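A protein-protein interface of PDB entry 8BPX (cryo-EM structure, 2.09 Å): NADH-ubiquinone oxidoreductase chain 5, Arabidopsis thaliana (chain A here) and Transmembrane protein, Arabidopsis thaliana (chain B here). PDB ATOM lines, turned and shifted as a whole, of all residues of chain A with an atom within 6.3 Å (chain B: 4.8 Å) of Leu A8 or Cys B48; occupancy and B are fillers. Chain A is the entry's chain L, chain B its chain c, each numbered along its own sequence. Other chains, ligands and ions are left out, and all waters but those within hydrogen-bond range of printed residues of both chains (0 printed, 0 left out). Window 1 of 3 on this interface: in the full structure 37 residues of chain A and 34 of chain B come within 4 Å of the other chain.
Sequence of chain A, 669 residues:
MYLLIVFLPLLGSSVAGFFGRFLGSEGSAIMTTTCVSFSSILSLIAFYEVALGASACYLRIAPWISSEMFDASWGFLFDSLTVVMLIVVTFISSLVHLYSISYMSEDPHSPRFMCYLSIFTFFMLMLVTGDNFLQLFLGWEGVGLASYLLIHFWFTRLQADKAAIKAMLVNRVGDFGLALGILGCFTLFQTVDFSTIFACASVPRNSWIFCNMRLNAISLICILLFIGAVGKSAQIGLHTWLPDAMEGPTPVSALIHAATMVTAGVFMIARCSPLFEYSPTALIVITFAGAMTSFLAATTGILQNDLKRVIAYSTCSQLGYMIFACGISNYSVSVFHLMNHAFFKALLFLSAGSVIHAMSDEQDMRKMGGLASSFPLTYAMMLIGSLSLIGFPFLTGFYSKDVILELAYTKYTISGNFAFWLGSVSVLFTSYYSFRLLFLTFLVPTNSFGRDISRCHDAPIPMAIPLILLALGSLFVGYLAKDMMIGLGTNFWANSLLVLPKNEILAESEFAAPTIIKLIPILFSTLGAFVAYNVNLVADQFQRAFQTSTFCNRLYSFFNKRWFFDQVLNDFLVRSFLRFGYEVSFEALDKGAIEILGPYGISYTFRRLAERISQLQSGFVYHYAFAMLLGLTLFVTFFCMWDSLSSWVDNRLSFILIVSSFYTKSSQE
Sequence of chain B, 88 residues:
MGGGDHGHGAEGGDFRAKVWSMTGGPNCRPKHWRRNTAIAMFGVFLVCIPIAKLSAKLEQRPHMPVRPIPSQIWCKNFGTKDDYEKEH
The backbone carbonyl oxygen (O) of Val B44 is in hydrogen-bond range of the side-chain sulfur (SG) of Cys B48 (3.5 Å).
Leu A3 touches Ile B51. Cys B48 touches Leu A4 (O to CD2, 3.7 Å). Leu A4 touches Ile B51 (CD2 to CG2, 3.7 Å). Leu A4 touches Ala B52 (CD1 to CB, 3.9 Å). SG of Cys B48 touches CD2 of Leu A8 (3.6 Å). CD2 of Leu A11 touches CG1 of Val B47, at 3.97 Å. CD1 of Leu A11 touches SG of Cys B48, at 3.6 Å. CG1 of Val B44 touches SG of Cys A35, 3.97 Å away.
Leu A8 touches one residue of chain B. Of the printed residues of chain B, Leu A3 touches Ile B51. Of the printed residues of chain A, Ala B52 touches Leu A4. Printed residues of chain A within 4 Å of Val B47: Leu A11. Printed residues of chain B within 4 Å of Leu A4: Cys B48, Ile B51 and Ala B52. Of the printed residues of chain B, Leu A11 touches Val B47 and Cys B48. Ile A5 touches none of the printed residues of chain B. Gly A12 touches none of the printed residues of chain B. The nearest residue of chain B that does not touch Leu A8 is Val B44 (4.3 Å).
Hydrophobic or aromatic side chains of chain A within 4 Å of the printed part of chain B: Leu A3, Leu A4, Leu A8 and Leu A11. Hydrophobic or aromatic side chains of chain B that line the printed part of chain A: Val B44, Val B47, Ile B51 and Ala B52. Among the printed residues, 8 pairs touch across the chains. Among the printed residues, no Asp or Glu carboxylate lies within 4 Å of a Lys or Arg side-chain nitrogen of the other chain.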
ATOM      1  N   LEU A   3       9.391  -2.193 -24.539  1.00  0.00           N
ATOM      2  CA  LEU A   3      10.117  -3.344 -25.062  1.00  0.00           C
ATOM      3  C   LEU A   3      10.062  -4.517 -24.089  1.00  0.00           C
ATOM      4  O   LEU A   3      10.010  -5.682 -24.507  1.00  0.00           O
ATOM      5  CB  LEU A   3      11.561  -2.950 -25.350  1.00  0.00           C
ATOM      6  CG  LEU A   3      11.832  -2.257 -26.684  1.00  0.00           C
ATOM      7  CD1 LEU A   3      13.321  -2.085 -26.899  1.00  0.00           C
ATOM      8  CD2 LEU A   3      11.196  -3.009 -27.831  1.00  0.00           C
ATOM      9  N   LEU A   4      10.079  -4.224 -22.785  1.00  0.00           N
ATOM     10  CA  LEU A   4      10.009  -5.278 -21.780  1.00  0.00           C
ATOM     11  C   LEU A   4       8.724  -6.079 -21.916  1.00  0.00           C
ATOM     12  O   LEU A   4       8.740  -7.308 -21.789  1.00  0.00           O
ATOM     13  CB  LEU A   4      10.125  -4.684 -20.374  1.00  0.00           C
ATOM     14  CG  LEU A   4      11.462  -4.069 -19.955  1.00  0.00           C
ATOM     15  CD1 LEU A   4      11.378  -3.523 -18.543  1.00  0.00           C
ATOM     16  CD2 LEU A   4      12.596  -5.084 -20.066  1.00  0.00           C
ATOM     17  N   ILE A   5       7.613  -5.404 -22.221  1.00  0.00           N
ATOM     18  CA  ILE A   5       6.333  -6.086 -22.399  1.00  0.00           C
ATOM     19  C   ILE A   5       6.463  -7.182 -23.448  1.00  0.00           C
ATOM     20  O   ILE A   5       6.028  -8.320 -23.248  1.00  0.00           O
ATOM     21  CB  ILE A   5       5.241  -5.079 -22.796  1.00  0.00           C
ATOM     22  CG1 ILE A   5       4.754  -4.277 -21.592  1.00  0.00           C
ATOM     23  CG2 ILE A   5       4.066  -5.789 -23.445  1.00  0.00           C
ATOM     24  CD1 ILE A   5       3.625  -3.343 -21.938  1.00  0.00           C
ATOM     25  N   VAL A   6       7.066  -6.846 -24.586  1.00  0.00           N
ATOM     26  CA  VAL A   6       7.133  -7.785 -25.696  1.00  0.00           C
ATOM     27  C   VAL A   6       8.149  -8.887 -25.416  1.00  0.00           C
ATOM     28  O   VAL A   6       7.887 -10.063 -25.681  1.00  0.00           O
ATOM     29  CB  VAL A   6       7.441  -7.036 -27.006  1.00  0.00           C
ATOM     30  CG1 VAL A   6       7.637  -8.017 -28.155  1.00  0.00           C
ATOM     31  CG2 VAL A   6       6.329  -6.050 -27.327  1.00  0.00           C
ATOM     32  N   PHE A   7       9.307  -8.535 -24.857  1.00  0.00           N
ATOM     33  CA  PHE A   7      10.426  -9.470 -24.823  1.00  0.00           C
ATOM     34  C   PHE A   7      10.558 -10.267 -23.527  1.00  0.00           C
ATOM     35  O   PHE A   7      11.331 -11.228 -23.501  1.00  0.00           O
ATOM     36  CB  PHE A   7      11.738  -8.729 -25.109  1.00  0.00           C
ATOM     37  CG  PHE A   7      11.891  -8.308 -26.544  1.00  0.00           C
ATOM     38  CD1 PHE A   7      12.201  -9.237 -27.524  1.00  0.00           C
ATOM     39  CD2 PHE A   7      11.704  -6.989 -26.918  1.00  0.00           C
ATOM     40  CE1 PHE A   7      12.337  -8.857 -28.846  1.00  0.00           C
ATOM     41  CE2 PHE A   7      11.836  -6.600 -28.240  1.00  0.00           C
ATOM     42  CZ  PHE A   7      12.151  -7.536 -29.204  1.00  0.00           C
ATOM     43  N   LEU A   8       9.825  -9.924 -22.466  1.00  0.00           N
ATOM     44  CA  LEU A   8       9.900 -10.712 -21.236  1.00  0.00           C
ATOM     45  C   LEU A   8       9.471 -12.166 -21.428  1.00  0.00           C
ATOM     46  O   LEU A   8      10.188 -13.065 -20.949  1.00  0.00           O
ATOM     47  CB  LEU A   8       9.082 -10.017 -20.141  1.00  0.00           C
ATOM     48  CG  LEU A   8       9.872  -9.130 -19.174  1.00  0.00           C
ATOM     49  CD1 LEU A   8       8.942  -8.450 -18.186  1.00  0.00           C
ATOM     50  CD2 LEU A   8      10.926  -9.943 -18.447  1.00  0.00           C
ATOM     51  N   PRO A   9       8.345 -12.476 -22.086  1.00  0.00           N
ATOM     52  CA  PRO A   9       8.023 -13.893 -22.326  1.00  0.00           C
ATOM     53  C   PRO A   9       9.064 -14.616 -23.163  1.00  0.00           C
ATOM     54  O   PRO A   9       9.285 -15.811 -22.946  1.00  0.00           O
ATOM     55  CB  PRO A   9       6.661 -13.842 -23.034  1.00  0.00           C
ATOM     56  CG  PRO A   9       6.171 -12.465 -22.885  1.00  0.00           C
ATOM     57  CD  PRO A   9       7.325 -11.578 -22.657  1.00  0.00           C
ATOM     58  N   LEU A  10       9.712 -13.931 -24.108  1.00  0.00           N
ATOM     59  CA  LEU A  10      10.809 -14.549 -24.845  1.00  0.00           C
ATOM     60  C   LEU A  10      11.948 -14.933 -23.911  1.00  0.00           C
ATOM     61  O   LEU A  10      12.509 -16.026 -24.024  1.00  0.00           O
ATOM     62  CB  LEU A  10      11.310 -13.610 -25.942  1.00  0.00           C
ATOM     63  CG  LEU A  10      12.461 -14.101 -26.833  1.00  0.00           C
ATOM     64  CD1 LEU A  10      12.196 -15.489 -27.411  1.00  0.00           C
ATOM     65  CD2 LEU A  10      12.772 -13.104 -27.930  1.00  0.00           C
ATOM     66  N   LEU A  11      12.297 -14.047 -22.975  1.00  0.00           N
ATOM     67  CA  LEU A  11      13.353 -14.349 -22.014  1.00  0.00           C
ATOM     68  C   LEU A  11      12.986 -15.553 -21.156  1.00  0.00           C
ATOM     69  O   LEU A  11      13.809 -16.452 -20.937  1.00  0.00           O
ATOM     70  CB  LEU A  11      13.619 -13.127 -21.136  1.00  0.00           C
ATOM     71  CG  LEU A  11      14.418 -11.994 -21.777  1.00  0.00           C
ATOM     72  CD1 LEU A  11      14.451 -10.785 -20.865  1.00  0.00           C
ATOM     73  CD2 LEU A  11      15.822 -12.453 -22.119  1.00  0.00           C
ATOM     74  N   GLY A  12      11.745 -15.585 -20.663  1.00  0.00           N
ATOM     75  CA  GLY A  12      11.314 -16.714 -19.860  1.00  0.00           C
ATOM     76  C   GLY A  12      11.339 -18.021 -20.629  1.00  0.00           C
ATOM     77  O   GLY A  12      11.814 -19.043 -20.124  1.00  0.00           O
ATOM     78  N   SER A  13      10.840 -18.003 -21.866  1.00  0.00           N
ATOM     79  CA  SER A  13      10.847 -19.201 -22.695  1.00  0.00           C
ATOM     80  C   SER A  13      12.273 -19.659 -22.977  1.00  0.00           C
ATOM     81  O   SER A  13      12.563 -20.860 -22.954  1.00  0.00           O
ATOM     82  CB  SER A  13      10.090 -18.935 -23.997  1.00  0.00           C
ATOM     83  OG  SER A  13      10.588 -19.710 -25.069  1.00  0.00           O
ATOM     84  N   THR A  34       6.530 -15.974 -13.784  1.00  0.00           N
ATOM     85  CA  THR A  34       7.027 -14.665 -13.317  1.00  0.00           C
ATOM     86  C   THR A  34       7.163 -13.736 -14.529  1.00  0.00           C
ATOM     87  O   THR A  34       6.444 -12.752 -14.542  1.00  0.00           O
ATOM     88  CB  THR A  34       8.305 -14.817 -12.451  1.00  0.00           C
ATOM     89  OG1 THR A  34       8.056 -15.564 -11.266  1.00  0.00           O
ATOM     90  CG2 THR A  34       8.923 -13.488 -12.072  1.00  0.00           C
ATOM     91  N   CYS A  35       7.978 -14.122 -15.513  1.00  0.00           N
ATOM     92  CA  CYS A  35       8.204 -13.299 -16.703  1.00  0.00           C
ATOM     93  C   CYS A  35       6.867 -12.919 -17.385  1.00  0.00           C
ATOM     94  O   CYS A  35       6.751 -11.731 -17.682  1.00  0.00           O
ATOM     95  CB  CYS A  35       9.255 -13.878 -17.672  1.00  0.00           C
ATOM     96  SG  CYS A  35      10.902 -14.169 -17.006  1.00  0.00           S
ATOM     97  N   VAL A  36       5.913 -13.843 -17.549  1.00  0.00           N
ATOM     98  CA  VAL A  36       4.662 -13.464 -18.197  1.00  0.00           C
ATOM     99  C   VAL A  36       3.826 -12.568 -17.282  1.00  0.00           C
ATOM    100  O   VAL A  36       3.181 -11.622 -17.746  1.00  0.00           O
ATOM    101  CB  VAL A  36       3.891 -14.717 -18.654  1.00  0.00           C
ATOM    102  CG1 VAL A  36       2.443 -14.386 -18.939  1.00  0.00           C
ATOM    103  CG2 VAL A  36       4.532 -15.305 -19.903  1.00  0.00           C
ATOM    104  N   PHE A  38       4.954 -10.430 -15.028  1.00  0.00           N
ATOM    105  CA  PHE A  38       5.542  -9.097 -15.056  1.00  0.00           C
ATOM    106  C   PHE A  38       5.179  -8.368 -16.341  1.00  0.00           C
ATOM    107  O   PHE A  38       4.894  -7.162 -16.326  1.00  0.00           O
ATOM    108  CB  PHE A  38       7.053  -9.187 -14.888  1.00  0.00           C
ATOM    109  CG  PHE A  38       7.509  -8.956 -13.488  1.00  0.00           C
ATOM    110  CD1 PHE A  38       7.443  -7.694 -12.928  1.00  0.00           C
ATOM    111  CD2 PHE A  38       7.981 -10.001 -12.717  1.00  0.00           C
ATOM    112  CE1 PHE A  38       7.854  -7.477 -11.634  1.00  0.00           C
ATOM    113  CE2 PHE A  38       8.392  -9.791 -11.424  1.00  0.00           C
ATOM    114  CZ  PHE A  38       8.331  -8.528 -10.882  1.00  0.00           C
ATOM    115  N   SER A  39       5.182  -9.089 -17.465  1.00  0.00           N
ATOM    116  CA  SER A  39       4.722  -8.496 -18.714  1.00  0.00           C
ATOM    117  C   SER A  39       3.261  -8.060 -18.609  1.00  0.00           C
ATOM    118  O   SER A  39       2.877  -7.021 -19.150  1.00  0.00           O
ATOM    119  CB  SER A  39       4.923  -9.482 -19.864  1.00  0.00           C
ATOM    120  OG  SER A  39       3.965  -9.295 -20.880  1.00  0.00           O
ATOM    121  N   LEU A  42       3.130  -4.769 -16.577  1.00  0.00           N
ATOM    122  CA  LEU A  42       3.541  -3.670 -17.440  1.00  0.00           C
ATOM    123  C   LEU A  42       2.487  -3.371 -18.498  1.00  0.00           C
ATOM    124  O   LEU A  42       2.325  -2.219 -18.902  1.00  0.00           O
ATOM    125  CB  LEU A  42       4.886  -3.986 -18.096  1.00  0.00           C
ATOM    126  CG  LEU A  42       6.099  -4.257 -17.206  1.00  0.00           C
ATOM    127  CD1 LEU A  42       7.340  -4.424 -18.061  1.00  0.00           C
ATOM    128  CD2 LEU A  42       6.301  -3.167 -16.166  1.00  0.00           C
ATOM    129  N   PHE A 122       4.941 -14.691 -26.649  1.00  0.00           N
ATOM    130  CA  PHE A 122       5.809 -13.713 -27.296  1.00  0.00           C
ATOM    131  C   PHE A 122       5.395 -13.475 -28.745  1.00  0.00           C
ATOM    132  O   PHE A 122       5.364 -12.327 -29.207  1.00  0.00           O
ATOM    133  CB  PHE A 122       7.267 -14.165 -27.226  1.00  0.00           C
ATOM    134  CG  PHE A 122       8.136 -13.557 -28.288  1.00  0.00           C
ATOM    135  CD1 PHE A 122       8.610 -12.262 -28.151  1.00  0.00           C
ATOM    136  CD2 PHE A 122       8.475 -14.273 -29.425  1.00  0.00           C
ATOM    137  CE1 PHE A 122       9.403 -11.694 -29.121  1.00  0.00           C
ATOM    138  CE2 PHE A 122       9.273 -13.710 -30.399  1.00  0.00           C
ATOM    139  CZ  PHE A 122       9.738 -12.416 -30.246  1.00  0.00           C
ATOM    140  N   VAL B  44      17.899 -12.836 -15.750  1.00  0.00           N
ATOM    141  CA  VAL B  44      16.825 -12.202 -16.540  1.00  0.00           C
ATOM    142  C   VAL B  44      16.748 -10.695 -16.134  1.00  0.00           C
ATOM    143  O   VAL B  44      16.801  -9.899 -17.044  1.00  0.00           O
ATOM    144  CB  VAL B  44      15.487 -12.986 -16.483  1.00  0.00           C
ATOM    145  CG1 VAL B  44      14.275 -12.094 -16.724  1.00  0.00           C
ATOM    146  CG2 VAL B  44      15.466 -14.235 -17.340  1.00  0.00           C
ATOM    147  N   PHE B  45      16.857 -10.348 -14.831  1.00  0.00           N
ATOM    148  CA  PHE B  45      16.799  -8.940 -14.440  1.00  0.00           C
ATOM    149  C   PHE B  45      17.971  -8.144 -15.024  1.00  0.00           C
ATOM    150  O   PHE B  45      17.788  -7.026 -15.543  1.00  0.00           O
ATOM    151  CB  PHE B  45      16.762  -8.834 -12.916  1.00  0.00           C
ATOM    152  CG  PHE B  45      17.041  -7.460 -12.397  1.00  0.00           C
ATOM    153  CD1 PHE B  45      18.282  -7.139 -11.879  1.00  0.00           C
ATOM    154  CD2 PHE B  45      16.062  -6.483 -12.434  1.00  0.00           C
ATOM    155  CE1 PHE B  45      18.538  -5.876 -11.407  1.00  0.00           C
ATOM    156  CE2 PHE B  45      16.316  -5.219 -11.962  1.00  0.00           C
ATOM    157  CZ  PHE B  45      17.556  -4.914 -11.447  1.00  0.00           C
ATOM    158  N   LEU B  46      19.180  -8.710 -14.962  1.00  0.00           N
ATOM    159  CA  LEU B  46      20.334  -8.028 -15.538  1.00  0.00           C
ATOM    160  C   LEU B  46      20.164  -7.813 -17.033  1.00  0.00           C
ATOM    161  O   LEU B  46      20.478  -6.736 -17.548  1.00  0.00           O
ATOM    162  CB  LEU B  46      21.612  -8.808 -15.264  1.00  0.00           C
ATOM    163  CG  LEU B  46      22.084  -8.787 -13.821  1.00  0.00           C
ATOM    164  CD1 LEU B  46      23.391  -9.538 -13.718  1.00  0.00           C
ATOM    165  CD2 LEU B  46      22.213  -7.351 -13.333  1.00  0.00           C
ATOM    166  N   VAL B  47      19.673  -8.827 -17.748  1.00  0.00           N
ATOM    167  CA  VAL B  47      19.424  -8.674 -19.178  1.00  0.00           C
ATOM    168  C   VAL B  47      18.339  -7.636 -19.433  1.00  0.00           C
ATOM    169  O   VAL B  47      18.361  -6.937 -20.452  1.00  0.00           O
ATOM    170  CB  VAL B  47      19.067 -10.041 -19.798  1.00  0.00           C
ATOM    171  CG1 VAL B  47      18.749  -9.908 -21.276  1.00  0.00           C
ATOM    172  CG2 VAL B  47      20.213 -11.012 -19.606  1.00  0.00           C
ATOM    173  N   CYS B  48      17.385  -7.505 -18.511  1.00  0.00           N
ATOM    174  CA  CYS B  48      16.272  -6.584 -18.718  1.00  0.00           C
ATOM    175  C   CYS B  48      16.689  -5.131 -18.553  1.00  0.00           C
ATOM    176  O   CYS B  48      16.042  -4.243 -19.118  1.00  0.00           O
ATOM    177  CB  CYS B  48      15.133  -6.911 -17.755  1.00  0.00           C
ATOM    178  SG  CYS B  48      14.059  -8.233 -18.314  1.00  0.00           S
ATOM    179  N   ILE B  49      17.730  -4.863 -17.769  1.00  0.00           N
ATOM    180  CA  ILE B  49      18.158  -3.469 -17.582  1.00  0.00           C
ATOM    181  C   ILE B  49      18.501  -2.781 -18.909  1.00  0.00           C
ATOM    182  O   ILE B  49      17.914  -1.724 -19.214  1.00  0.00           O
ATOM    183  CB  ILE B  49      19.332  -3.372 -16.593  1.00  0.00           C
ATOM    184  CG1 ILE B  49      18.855  -3.618 -15.161  1.00  0.00           C
ATOM    185  CG2 ILE B  49      20.037  -2.027 -16.711  1.00  0.00           C
ATOM    186  CD1 ILE B  49      19.864  -4.322 -14.307  1.00  0.00           C
ATOM    187  N   PRO B  50      19.414  -3.312 -19.737  1.00  0.00           N
ATOM    188  CA  PRO B  50      19.704  -2.633 -21.012  1.00  0.00           C
ATOM    189  C   PRO B  50      18.510  -2.557 -21.943  1.00  0.00           C
ATOM    190  O   PRO B  50      18.379  -1.575 -22.686  1.00  0.00           O
ATOM    191  CB  PRO B  50      20.831  -3.483 -21.616  1.00  0.00           C
ATOM    192  CG  PRO B  50      21.395  -4.232 -20.482  1.00  0.00           C
ATOM    193  CD  PRO B  50      20.244  -4.522 -19.600  1.00  0.00           C
ATOM    194  N   ILE B  51      17.641  -3.568 -21.931  1.00  0.00           N
ATOM    195  CA  ILE B  51      16.442  -3.518 -22.760  1.00  0.00           C
ATOM    196  C   ILE B  51      15.565  -2.346 -22.344  1.00  0.00           C
ATOM    197  O   ILE B  51      15.033  -1.620 -23.190  1.00  0.00           O
ATOM    198  CB  ILE B  51      15.675  -4.852 -22.687  1.00  0.00           C
ATOM    199  CG1 ILE B  51      16.460  -5.970 -23.373  1.00  0.00           C
ATOM    200  CG2 ILE B  51      14.305  -4.721 -23.328  1.00  0.00           C
ATOM    201  CD1 ILE B  51      15.809  -7.332 -23.235  1.00  0.00           C
ATOM    202  N   ALA B  52      15.404  -2.144 -21.034  1.00  0.00           N
ATOM    203  CA  ALA B  52      14.605  -1.025 -20.549  1.00  0.00           C
ATOM    204  C   ALA B  52      15.229   0.311 -20.937  1.00  0.00           C
ATOM    205  O   ALA B  52      14.518   1.240 -21.336  1.00  0.00           O
ATOM    206  CB  ALA B  52      14.427  -1.120 -19.035  1.00  0.00           C
